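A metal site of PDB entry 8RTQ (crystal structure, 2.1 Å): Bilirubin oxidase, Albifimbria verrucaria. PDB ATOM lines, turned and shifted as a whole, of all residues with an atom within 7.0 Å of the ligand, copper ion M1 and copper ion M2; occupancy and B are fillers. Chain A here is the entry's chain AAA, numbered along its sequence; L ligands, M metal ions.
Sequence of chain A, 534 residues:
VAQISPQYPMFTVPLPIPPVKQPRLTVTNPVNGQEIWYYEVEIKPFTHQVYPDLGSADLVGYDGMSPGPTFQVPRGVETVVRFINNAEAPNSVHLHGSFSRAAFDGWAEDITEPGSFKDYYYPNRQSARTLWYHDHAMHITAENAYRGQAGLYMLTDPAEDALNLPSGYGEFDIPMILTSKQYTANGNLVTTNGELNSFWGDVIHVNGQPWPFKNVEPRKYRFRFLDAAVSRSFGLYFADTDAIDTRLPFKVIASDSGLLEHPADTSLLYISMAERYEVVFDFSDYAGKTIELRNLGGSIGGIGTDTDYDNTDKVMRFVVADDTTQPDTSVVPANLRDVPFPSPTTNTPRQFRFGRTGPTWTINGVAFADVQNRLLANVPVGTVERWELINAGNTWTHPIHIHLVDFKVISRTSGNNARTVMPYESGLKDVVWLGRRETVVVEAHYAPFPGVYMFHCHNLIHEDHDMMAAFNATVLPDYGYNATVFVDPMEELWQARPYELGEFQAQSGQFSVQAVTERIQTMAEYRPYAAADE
O2 of the ligand lies close to NE2 of His 401, 3.3 Å away.
Residues that only touch the ligand: His 94 (3.4 Å).
Of the 25 residues printed, 8 come within 4 Å of the ligand.
Along chain A the residues within 4 Å of the ligand span positions 94 to 458.
Copper ion M1 is bound by a ring nitrogen (ND1) of His 96 (2.0 Å), a ring nitrogen (NE2) of His 134 (2.1 Å), a ring nitrogen (NE2) of His 458 (2.2 Å) and an oxygen (O1) of the ligand (2.5 Å).
Copper ion M2 is bound by a ring nitrogen (NE2) of His 403 (2.0 Å).
A ring nitrogen (NE2) of His 136 binds copper ion M2 (2.0 Å).
NE2 of His 456 binds copper ion M2 (2.2 Å).
Copper ion M2 is bound by O2 of the ligand (2.4 Å).
Copper ion M2 has four donor atoms within binding distance.
His 94 touches copper ion M1 (CD2 to CU, 3.9 Å).
CZ2 of Trp 132 touches copper ion M1, 3.7 Å away.
Of the 25 residues printed, 5 come within 4 Å of copper ion M1.
Along chain A the residues within 4 Å of copper ion M1 span positions 94 to 458.
The backbone NH (N) of His 403 lies within hydrogen-bond range of the backbone carbonyl oxygen (O) of Met 454, at 3.2 Å.
The side-chain carboxylate (OD2) of Asp 105 sits at hydrogen-bond distance from a ring nitrogen (ND1) of His 403 (2.7 Å).
OG1 of Thr 141 lies close to O of His 136 (3.3 Å).
ND1 of His 401 lies close to NE2 of His 96 (3.4 Å).
N of His 96 sits close to NE2 of His 94 (3.4 Å).
The backbone NH of His 96 lies within hydrogen-bond range of the backbone carbonyl oxygen of Trp 132 (2.8 Å).
The guanidinium group of Arg 276 sits at hydrogen-bond distance from a ring nitrogen (NE2) of His 96 (3.3 Å).
The backbone carbonyl oxygen (O) of His 456 lies within hydrogen-bond range of the backbone NH (N) of His 401 (2.8 Å).
His 401 touches copper ion M2.
Within 4 Å of copper ion M2: His 136, His 401, His 403 and His 456.
The nearest printed residue that does not touch copper ion M2 is Met 454 (4.1 Å).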
ATOM      1  N   HIS A  94     -12.085  28.032 -19.192  1.00  0.00           N
ATOM      2  CA  HIS A  94     -11.641  29.151 -18.317  1.00  0.00           C
ATOM      3  C   HIS A  94     -10.109  29.189 -18.279  1.00  0.00           C
ATOM      4  O   HIS A  94      -9.497  28.148 -17.986  1.00  0.00           O
ATOM      5  CB  HIS A  94     -12.183  28.950 -16.917  1.00  0.00           C
ATOM      6  CG  HIS A  94     -11.572  29.886 -15.943  1.00  0.00           C
ATOM      7  ND1 HIS A  94     -11.698  31.255 -16.074  1.00  0.00           N
ATOM      8  CD2 HIS A  94     -10.940  29.674 -14.772  1.00  0.00           C
ATOM      9  CE1 HIS A  94     -11.110  31.836 -15.041  1.00  0.00           C
ATOM     10  NE2 HIS A  94     -10.642  30.890 -14.235  1.00  0.00           N
ATOM     11  N   LEU A  95      -9.521  30.349 -18.578  1.00  0.00           N
ATOM     12  CA  LEU A  95      -8.084  30.637 -18.315  1.00  0.00           C
ATOM     13  C   LEU A  95      -7.989  31.164 -16.892  1.00  0.00           C
ATOM     14  O   LEU A  95      -8.225  32.350 -16.650  1.00  0.00           O
ATOM     15  CB  LEU A  95      -7.546  31.643 -19.339  1.00  0.00           C
ATOM     16  CG  LEU A  95      -6.045  31.924 -19.261  1.00  0.00           C
ATOM     17  CD1 LEU A  95      -5.274  30.629 -19.356  1.00  0.00           C
ATOM     18  CD2 LEU A  95      -5.596  32.857 -20.382  1.00  0.00           C
ATOM     19  N   HIS A  96      -7.728  30.268 -15.968  1.00  0.00           N
ATOM     20  CA  HIS A  96      -7.502  30.574 -14.540  1.00  0.00           C
ATOM     21  C   HIS A  96      -6.217  31.403 -14.368  1.00  0.00           C
ATOM     22  O   HIS A  96      -5.116  30.896 -14.688  1.00  0.00           O
ATOM     23  CB  HIS A  96      -7.539  29.257 -13.748  1.00  0.00           C
ATOM     24  CG  HIS A  96      -7.594  29.431 -12.275  1.00  0.00           C
ATOM     25  ND1 HIS A  96      -8.361  28.646 -11.488  1.00  0.00           N
ATOM     26  CD2 HIS A  96      -6.963  30.303 -11.458  1.00  0.00           C
ATOM     27  CE1 HIS A  96      -8.200  28.992 -10.228  1.00  0.00           C
ATOM     28  NE2 HIS A  96      -7.350  30.016 -10.179  1.00  0.00           N
ATOM     29  N   GLY A  97      -6.349  32.621 -13.831  1.00  0.00           N
ATOM     30  CA  GLY A  97      -5.246  33.551 -13.570  1.00  0.00           C
ATOM     31  C   GLY A  97      -5.226  34.715 -14.543  1.00  0.00           C
ATOM     32  O   GLY A  97      -4.336  35.562 -14.415  1.00  0.00           O
ATOM     33  N   ASP A 105     -14.295  34.242 -20.201  1.00  0.00           N
ATOM     34  CA  ASP A 105     -13.726  33.822 -18.890  1.00  0.00           C
ATOM     35  C   ASP A 105     -14.137  32.410 -18.508  1.00  0.00           C
ATOM     36  O   ASP A 105     -13.637  31.918 -17.480  1.00  0.00           O
ATOM     37  CB  ASP A 105     -14.129  34.809 -17.786  1.00  0.00           C
ATOM     38  CG  ASP A 105     -13.343  34.628 -16.501  1.00  0.00           C
ATOM     39  OD1 ASP A 105     -12.107  34.483 -16.575  1.00  0.00           O
ATOM     40  OD2 ASP A 105     -14.009  34.665 -15.414  1.00  0.00           O
ATOM     41  N   GLY A 106     -15.014  31.766 -19.288  1.00  0.00           N
ATOM     42  CA  GLY A 106     -15.546  30.420 -19.012  1.00  0.00           C
ATOM     43  C   GLY A 106     -16.690  30.427 -17.992  1.00  0.00           C
ATOM     44  O   GLY A 106     -16.815  29.461 -17.220  1.00  0.00           O
ATOM     45  N   TRP A 132      -3.461  28.418 -15.868  1.00  0.00           N
ATOM     46  CA  TRP A 132      -3.844  27.104 -16.415  1.00  0.00           C
ATOM     47  C   TRP A 132      -5.254  27.278 -16.969  1.00  0.00           C
ATOM     48  O   TRP A 132      -5.975  28.214 -16.506  1.00  0.00           O
ATOM     49  CB  TRP A 132      -3.660  26.008 -15.356  1.00  0.00           C
ATOM     50  CG  TRP A 132      -4.596  26.053 -14.175  1.00  0.00           C
ATOM     51  CD1 TRP A 132      -4.730  27.052 -13.243  1.00  0.00           C
ATOM     52  CD2 TRP A 132      -5.453  24.982 -13.733  1.00  0.00           C
ATOM     53  NE1 TRP A 132      -5.627  26.688 -12.291  1.00  0.00           N
ATOM     54  CE2 TRP A 132      -6.104  25.426 -12.566  1.00  0.00           C
ATOM     55  CE3 TRP A 132      -5.737  23.695 -14.223  1.00  0.00           C
ATOM     56  CZ2 TRP A 132      -6.997  24.621 -11.871  1.00  0.00           C
ATOM     57  CZ3 TRP A 132      -6.637  22.909 -13.552  1.00  0.00           C
ATOM     58  CH2 TRP A 132      -7.277  23.383 -12.398  1.00  0.00           C
ATOM     59  N   HIS A 134      -8.816  25.257 -18.176  1.00  0.00           N
ATOM     60  CA  HIS A 134      -9.554  24.016 -17.837  1.00  0.00           C
ATOM     61  C   HIS A 134     -11.046  24.227 -18.019  1.00  0.00           C
ATOM     62  O   HIS A 134     -11.550  25.427 -18.134  1.00  0.00           O
ATOM     63  CB  HIS A 134      -9.214  23.576 -16.418  1.00  0.00           C
ATOM     64  CG  HIS A 134      -9.624  24.541 -15.374  1.00  0.00           C
ATOM     65  ND1 HIS A 134     -10.920  24.617 -14.927  1.00  0.00           N
ATOM     66  CD2 HIS A 134      -8.921  25.430 -14.659  1.00  0.00           C
ATOM     67  CE1 HIS A 134     -11.012  25.518 -13.973  1.00  0.00           C
ATOM     68  NE2 HIS A 134      -9.798  26.040 -13.781  1.00  0.00           N
ATOM     69  N   ASP A 135     -11.746  23.101 -17.990  1.00  0.00           N
ATOM     70  CA  ASP A 135     -13.175  23.125 -18.271  1.00  0.00           C
ATOM     71  C   ASP A 135     -13.897  23.738 -17.074  1.00  0.00           C
ATOM     72  O   ASP A 135     -13.364  23.665 -15.955  1.00  0.00           O
ATOM     73  CB  ASP A 135     -13.717  21.751 -18.618  1.00  0.00           C
ATOM     74  CG  ASP A 135     -15.132  21.918 -19.130  1.00  0.00           C
ATOM     75  OD1 ASP A 135     -15.242  22.567 -20.191  1.00  0.00           O
ATOM     76  OD2 ASP A 135     -16.068  21.537 -18.383  1.00  0.00           O
ATOM     77  N   HIS A 136     -15.017  24.386 -17.357  1.00  0.00           N
ATOM     78  CA  HIS A 136     -15.852  25.059 -16.333  1.00  0.00           C
ATOM     79  C   HIS A 136     -17.354  24.870 -16.636  1.00  0.00           C
ATOM     80  O   HIS A 136     -18.167  25.594 -16.018  1.00  0.00           O
ATOM     81  CB  HIS A 136     -15.412  26.521 -16.325  1.00  0.00           C
ATOM     82  CG  HIS A 136     -15.470  27.186 -14.988  1.00  0.00           C
ATOM     83  ND1 HIS A 136     -16.598  27.162 -14.208  1.00  0.00           N
ATOM     84  CD2 HIS A 136     -14.518  27.878 -14.301  1.00  0.00           C
ATOM     85  CE1 HIS A 136     -16.350  27.810 -13.081  1.00  0.00           C
ATOM     86  NE2 HIS A 136     -15.088  28.269 -13.113  1.00  0.00           N
ATOM     87  N   THR A 141     -18.005  20.044 -14.491  1.00  0.00           N
ATOM     88  CA  THR A 141     -16.631  20.560 -14.447  1.00  0.00           C
ATOM     89  C   THR A 141     -15.696  19.482 -13.867  1.00  0.00           C
ATOM     90  O   THR A 141     -14.628  19.231 -14.456  1.00  0.00           O
ATOM     91  CB  THR A 141     -16.570  21.877 -13.693  1.00  0.00           C
ATOM     92  OG1 THR A 141     -17.280  22.871 -14.428  1.00  0.00           O
ATOM     93  CG2 THR A 141     -15.145  22.332 -13.465  1.00  0.00           C
ATOM     94  N   ALA A 274      -6.194  24.214  -7.430  1.00  0.00           N
ATOM     95  CA  ALA A 274      -6.122  25.355  -8.367  1.00  0.00           C
ATOM     96  C   ALA A 274      -5.000  26.320  -7.956  1.00  0.00           C
ATOM     97  O   ALA A 274      -4.698  27.223  -8.728  1.00  0.00           O
ATOM     98  CB  ALA A 274      -7.466  26.051  -8.485  1.00  0.00           C
ATOM     99  N   ARG A 276      -1.253  27.501  -7.762  1.00  0.00           N
ATOM    100  CA  ARG A 276       0.094  27.391  -8.392  1.00  0.00           C
ATOM    101  C   ARG A 276       1.135  27.955  -7.411  1.00  0.00           C
ATOM    102  O   ARG A 276       0.946  29.082  -6.886  1.00  0.00           O
ATOM    103  CB  ARG A 276       0.164  28.112  -9.749  1.00  0.00           C
ATOM    104  CG  ARG A 276      -0.706  27.486 -10.814  1.00  0.00           C
ATOM    105  CD  ARG A 276      -2.134  27.963 -10.674  1.00  0.00           C
ATOM    106  NE  ARG A 276      -2.256  29.366 -11.074  1.00  0.00           N
ATOM    107  CZ  ARG A 276      -3.205  30.186 -10.624  1.00  0.00           C
ATOM    108  NH1 ARG A 276      -3.213  31.455 -11.027  1.00  0.00           N
ATOM    109  NH2 ARG A 276      -4.120  29.762  -9.756  1.00  0.00           N
ATOM    110  N   HIS A 401     -11.772  30.521  -4.673  1.00  0.00           N
ATOM    111  CA  HIS A 401     -11.249  31.196  -5.878  1.00  0.00           C
ATOM    112  C   HIS A 401     -12.230  32.293  -6.260  1.00  0.00           C
ATOM    113  O   HIS A 401     -13.443  32.050  -6.233  1.00  0.00           O
ATOM    114  CB  HIS A 401     -11.092  30.186  -7.012  1.00  0.00           C
ATOM    115  CG  HIS A 401     -10.659  30.797  -8.289  1.00  0.00           C
ATOM    116  ND1 HIS A 401      -9.628  31.722  -8.361  1.00  0.00           N
ATOM    117  CD2 HIS A 401     -11.113  30.618  -9.556  1.00  0.00           C
ATOM    118  CE1 HIS A 401      -9.432  32.052  -9.633  1.00  0.00           C
ATOM    119  NE2 HIS A 401     -10.357  31.395 -10.387  1.00  0.00           N
ATOM    120  N   ILE A 402     -11.688  33.457  -6.603  1.00  0.00           N
ATOM    121  CA  ILE A 402     -12.438  34.628  -7.117  1.00  0.00           C
ATOM    122  C   ILE A 402     -11.873  34.928  -8.496  1.00  0.00           C
ATOM    123  O   ILE A 402     -10.677  35.243  -8.602  1.00  0.00           O
ATOM    124  CB  ILE A 402     -12.272  35.813  -6.159  1.00  0.00           C
ATOM    125  CG1 ILE A 402     -12.621  35.437  -4.715  1.00  0.00           C
ATOM    126  CG2 ILE A 402     -13.091  37.006  -6.664  1.00  0.00           C
ATOM    127  CD1 ILE A 402     -12.243  36.499  -3.666  1.00  0.00           C
ATOM    128  N   HIS A 403     -12.728  34.877  -9.508  1.00  0.00           N
ATOM    129  CA  HIS A 403     -12.388  35.255 -10.906  1.00  0.00           C
ATOM    130  C   HIS A 403     -12.037  36.757 -10.976  1.00  0.00           C
ATOM    131  O   HIS A 403     -12.314  37.473 -10.023  1.00  0.00           O
ATOM    132  CB  HIS A 403     -13.554  34.900 -11.854  1.00  0.00           C
ATOM    133  CG  HIS A 403     -13.686  33.443 -12.097  1.00  0.00           C
ATOM    134  ND1 HIS A 403     -13.635  32.921 -13.350  1.00  0.00           N
ATOM    135  CD2 HIS A 403     -13.876  32.397 -11.256  1.00  0.00           C
ATOM    136  CE1 HIS A 403     -13.804  31.611 -13.297  1.00  0.00           C
ATOM    137  NE2 HIS A 403     -13.948  31.250 -12.023  1.00  0.00           N
ATOM    138  N   VAL A 431      -6.524  31.876  -5.421  1.00  0.00           N
ATOM    139  CA  VAL A 431      -7.147  30.800  -4.612  1.00  0.00           C
ATOM    140  C   VAL A 431      -6.586  30.867  -3.189  1.00  0.00           C
ATOM    141  O   VAL A 431      -5.410  31.134  -3.028  1.00  0.00           O
ATOM    142  CB  VAL A 431      -6.858  29.430  -5.242  1.00  0.00           C
ATOM    143  CG1 VAL A 431      -7.515  28.282  -4.475  1.00  0.00           C
ATOM    144  CG2 VAL A 431      -7.282  29.417  -6.702  1.00  0.00           C
ATOM    145  N   MET A 454     -17.612  34.723 -11.578  1.00  0.00           N
ATOM    146  CA  MET A 454     -17.873  33.617 -10.639  1.00  0.00           C
ATOM    147  C   MET A 454     -16.863  33.699  -9.514  1.00  0.00           C
ATOM    148  O   MET A 454     -15.834  34.343  -9.666  1.00  0.00           O
ATOM    149  CB  MET A 454     -17.746  32.276 -11.370  1.00  0.00           C
ATOM    150  CG  MET A 454     -18.788  32.128 -12.491  1.00  0.00           C
ATOM    151  SD  MET A 454     -18.628  30.550 -13.356  1.00  0.00           S
ATOM    152  CE  MET A 454     -17.020  30.762 -14.098  1.00  0.00           C
ATOM    153  N   PHE A 455     -17.242  33.193  -8.349  1.00  0.00           N
ATOM    154  CA  PHE A 455     -16.335  32.827  -7.238  1.00  0.00           C
ATOM    155  C   PHE A 455     -16.958  31.573  -6.623  1.00  0.00           C
ATOM    156  O   PHE A 455     -18.178  31.357  -6.747  1.00  0.00           O
ATOM    157  CB  PHE A 455     -16.138  33.956  -6.230  1.00  0.00           C
ATOM    158  CG  PHE A 455     -17.329  34.319  -5.375  1.00  0.00           C
ATOM    159  CD1 PHE A 455     -18.386  35.059  -5.894  1.00  0.00           C
ATOM    160  CD2 PHE A 455     -17.383  33.950  -4.045  1.00  0.00           C
ATOM    161  CE1 PHE A 455     -19.463  35.415  -5.105  1.00  0.00           C
ATOM    162  CE2 PHE A 455     -18.447  34.334  -3.237  1.00  0.00           C
ATOM    163  CZ  PHE A 455     -19.494  35.071  -3.770  1.00  0.00           C
ATOM    164  N   HIS A 456     -16.113  30.711  -6.089  1.00  0.00           N
ATOM    165  CA  HIS A 456     -16.523  29.360  -5.718  1.00  0.00           C
ATOM    166  C   HIS A 456     -15.383  28.662  -5.026  1.00  0.00           C
ATOM    167  O   HIS A 456     -14.214  29.141  -5.089  1.00  0.00           O
ATOM    168  CB  HIS A 456     -16.936  28.579  -6.961  1.00  0.00           C
ATOM    169  CG  HIS A 456     -15.873  28.489  -7.998  1.00  0.00           C
ATOM    170  ND1 HIS A 456     -15.009  27.439  -8.084  1.00  0.00           N
ATOM    171  CD2 HIS A 456     -15.547  29.337  -8.998  1.00  0.00           C
ATOM    172  CE1 HIS A 456     -14.224  27.605  -9.120  1.00  0.00           C
ATOM    173  NE2 HIS A 456     -14.528  28.779  -9.689  1.00  0.00           N
ATOM    174  N   CYS A 457     -15.748  27.559  -4.412  1.00  0.00           N
ATOM    175  CA  CYS A 457     -14.802  26.510  -4.007  1.00  0.00           C
ATOM    176  C   CYS A 457     -14.264  25.833  -5.281  1.00  0.00           C
ATOM    177  O   CYS A 457     -15.072  25.610  -6.223  1.00  0.00           O
ATOM    178  CB  CYS A 457     -15.477  25.570  -3.022  1.00  0.00           C
ATOM    179  SG  CYS A 457     -14.341  24.263  -2.537  1.00  0.00           S
ATOM    180  N   HIS A 458     -12.980  25.471  -5.312  1.00  0.00           N
ATOM    181  CA  HIS A 458     -12.319  24.766  -6.434  1.00  0.00           C
ATOM    182  C   HIS A 458     -12.094  23.292  -6.089  1.00  0.00           C
ATOM    183  O   HIS A 458     -11.426  22.589  -6.911  1.00  0.00           O
ATOM    184  CB  HIS A 458     -11.028  25.491  -6.850  1.00  0.00           C
ATOM    185  CG  HIS A 458     -10.722  25.425  -8.306  1.00  0.00           C
ATOM    186  ND1 HIS A 458     -10.386  24.245  -8.929  1.00  0.00           N
ATOM    187  CD2 HIS A 458     -10.631  26.403  -9.240  1.00  0.00           C
ATOM    188  CE1 HIS A 458     -10.156  24.497 -10.203  1.00  0.00           C
ATOM    189  NE2 HIS A 458     -10.291  25.808 -10.418  1.00  0.00           N
ATOM    190  N   LEU A 460     -13.834  20.373  -7.064  1.00  0.00           N
ATOM    191  CA  LEU A 460     -14.700  20.424  -8.251  1.00  0.00           C
ATOM    192  C   LEU A 460     -16.018  19.696  -7.929  1.00  0.00           C
ATOM    193  O   LEU A 460     -17.048  20.053  -8.558  1.00  0.00           O
ATOM    194  CB  LEU A 460     -13.981  19.846  -9.479  1.00  0.00           C
ATOM    195  CG  LEU A 460     -12.700  20.574  -9.881  1.00  0.00           C
ATOM    196  CD1 LEU A 460     -12.079  19.914 -11.088  1.00  0.00           C
ATOM    197  CD2 LEU A 460     -12.971  22.038 -10.179  1.00  0.00           C
ATOM    198  N   GLU A 463     -17.984  22.376  -6.202  1.00  0.00           N
ATOM    199  CA  GLU A 463     -18.301  23.400  -7.232  1.00  0.00           C
ATOM    200  C   GLU A 463     -19.509  22.930  -8.064  1.00  0.00           C
ATOM    201  O   GLU A 463     -20.380  23.737  -8.289  1.00  0.00           O
ATOM    202  CB  GLU A 463     -17.076  23.596  -8.118  1.00  0.00           C
ATOM    203  CG  GLU A 463     -17.186  24.784  -9.049  1.00  0.00           C
ATOM    204  CD  GLU A 463     -16.019  24.883 -10.014  1.00  0.00           C
ATOM    205  OE1 GLU A 463     -14.844  24.735  -9.550  1.00  0.00           O
ATOM    206  OE2 GLU A 463     -16.299  25.135 -11.231  1.00  0.00           O
ATOM    207  N   MET A 468     -20.906  27.709  -5.669  1.00  0.00           N
ATOM    208  CA  MET A 468     -20.475  28.730  -6.636  1.00  0.00           C
ATOM    209  C   MET A 468     -21.531  29.824  -6.737  1.00  0.00           C
ATOM    210  O   MET A 468     -22.730  29.510  -6.663  1.00  0.00           O
ATOM    211  CB  MET A 468     -20.263  28.073  -7.997  1.00  0.00           C
ATOM    212  CG  MET A 468     -19.682  28.996  -9.059  1.00  0.00           C
ATOM    213  SD  MET A 468     -18.971  27.953 -10.387  1.00  0.00           S
ATOM    214  CE  MET A 468     -20.454  27.418 -11.248  1.00  0.00           C
HETATM  215  O1  LIG L   1     -12.085  27.790 -12.214  1.00  0.00           O
HETATM  216  O2  LIG L   1     -11.700  28.666 -11.632  1.00  0.00           O
HETATM  217 CU    CU M   1      -9.648  27.166 -12.034  1.00  0.00          CU
HETATM  218 CU    CU M   2     -14.004  29.283 -11.731  1.00  0.00          CU
HETATM  219 CU    CU M   3     -10.528  31.053 -12.290  1.00  0.00          CU
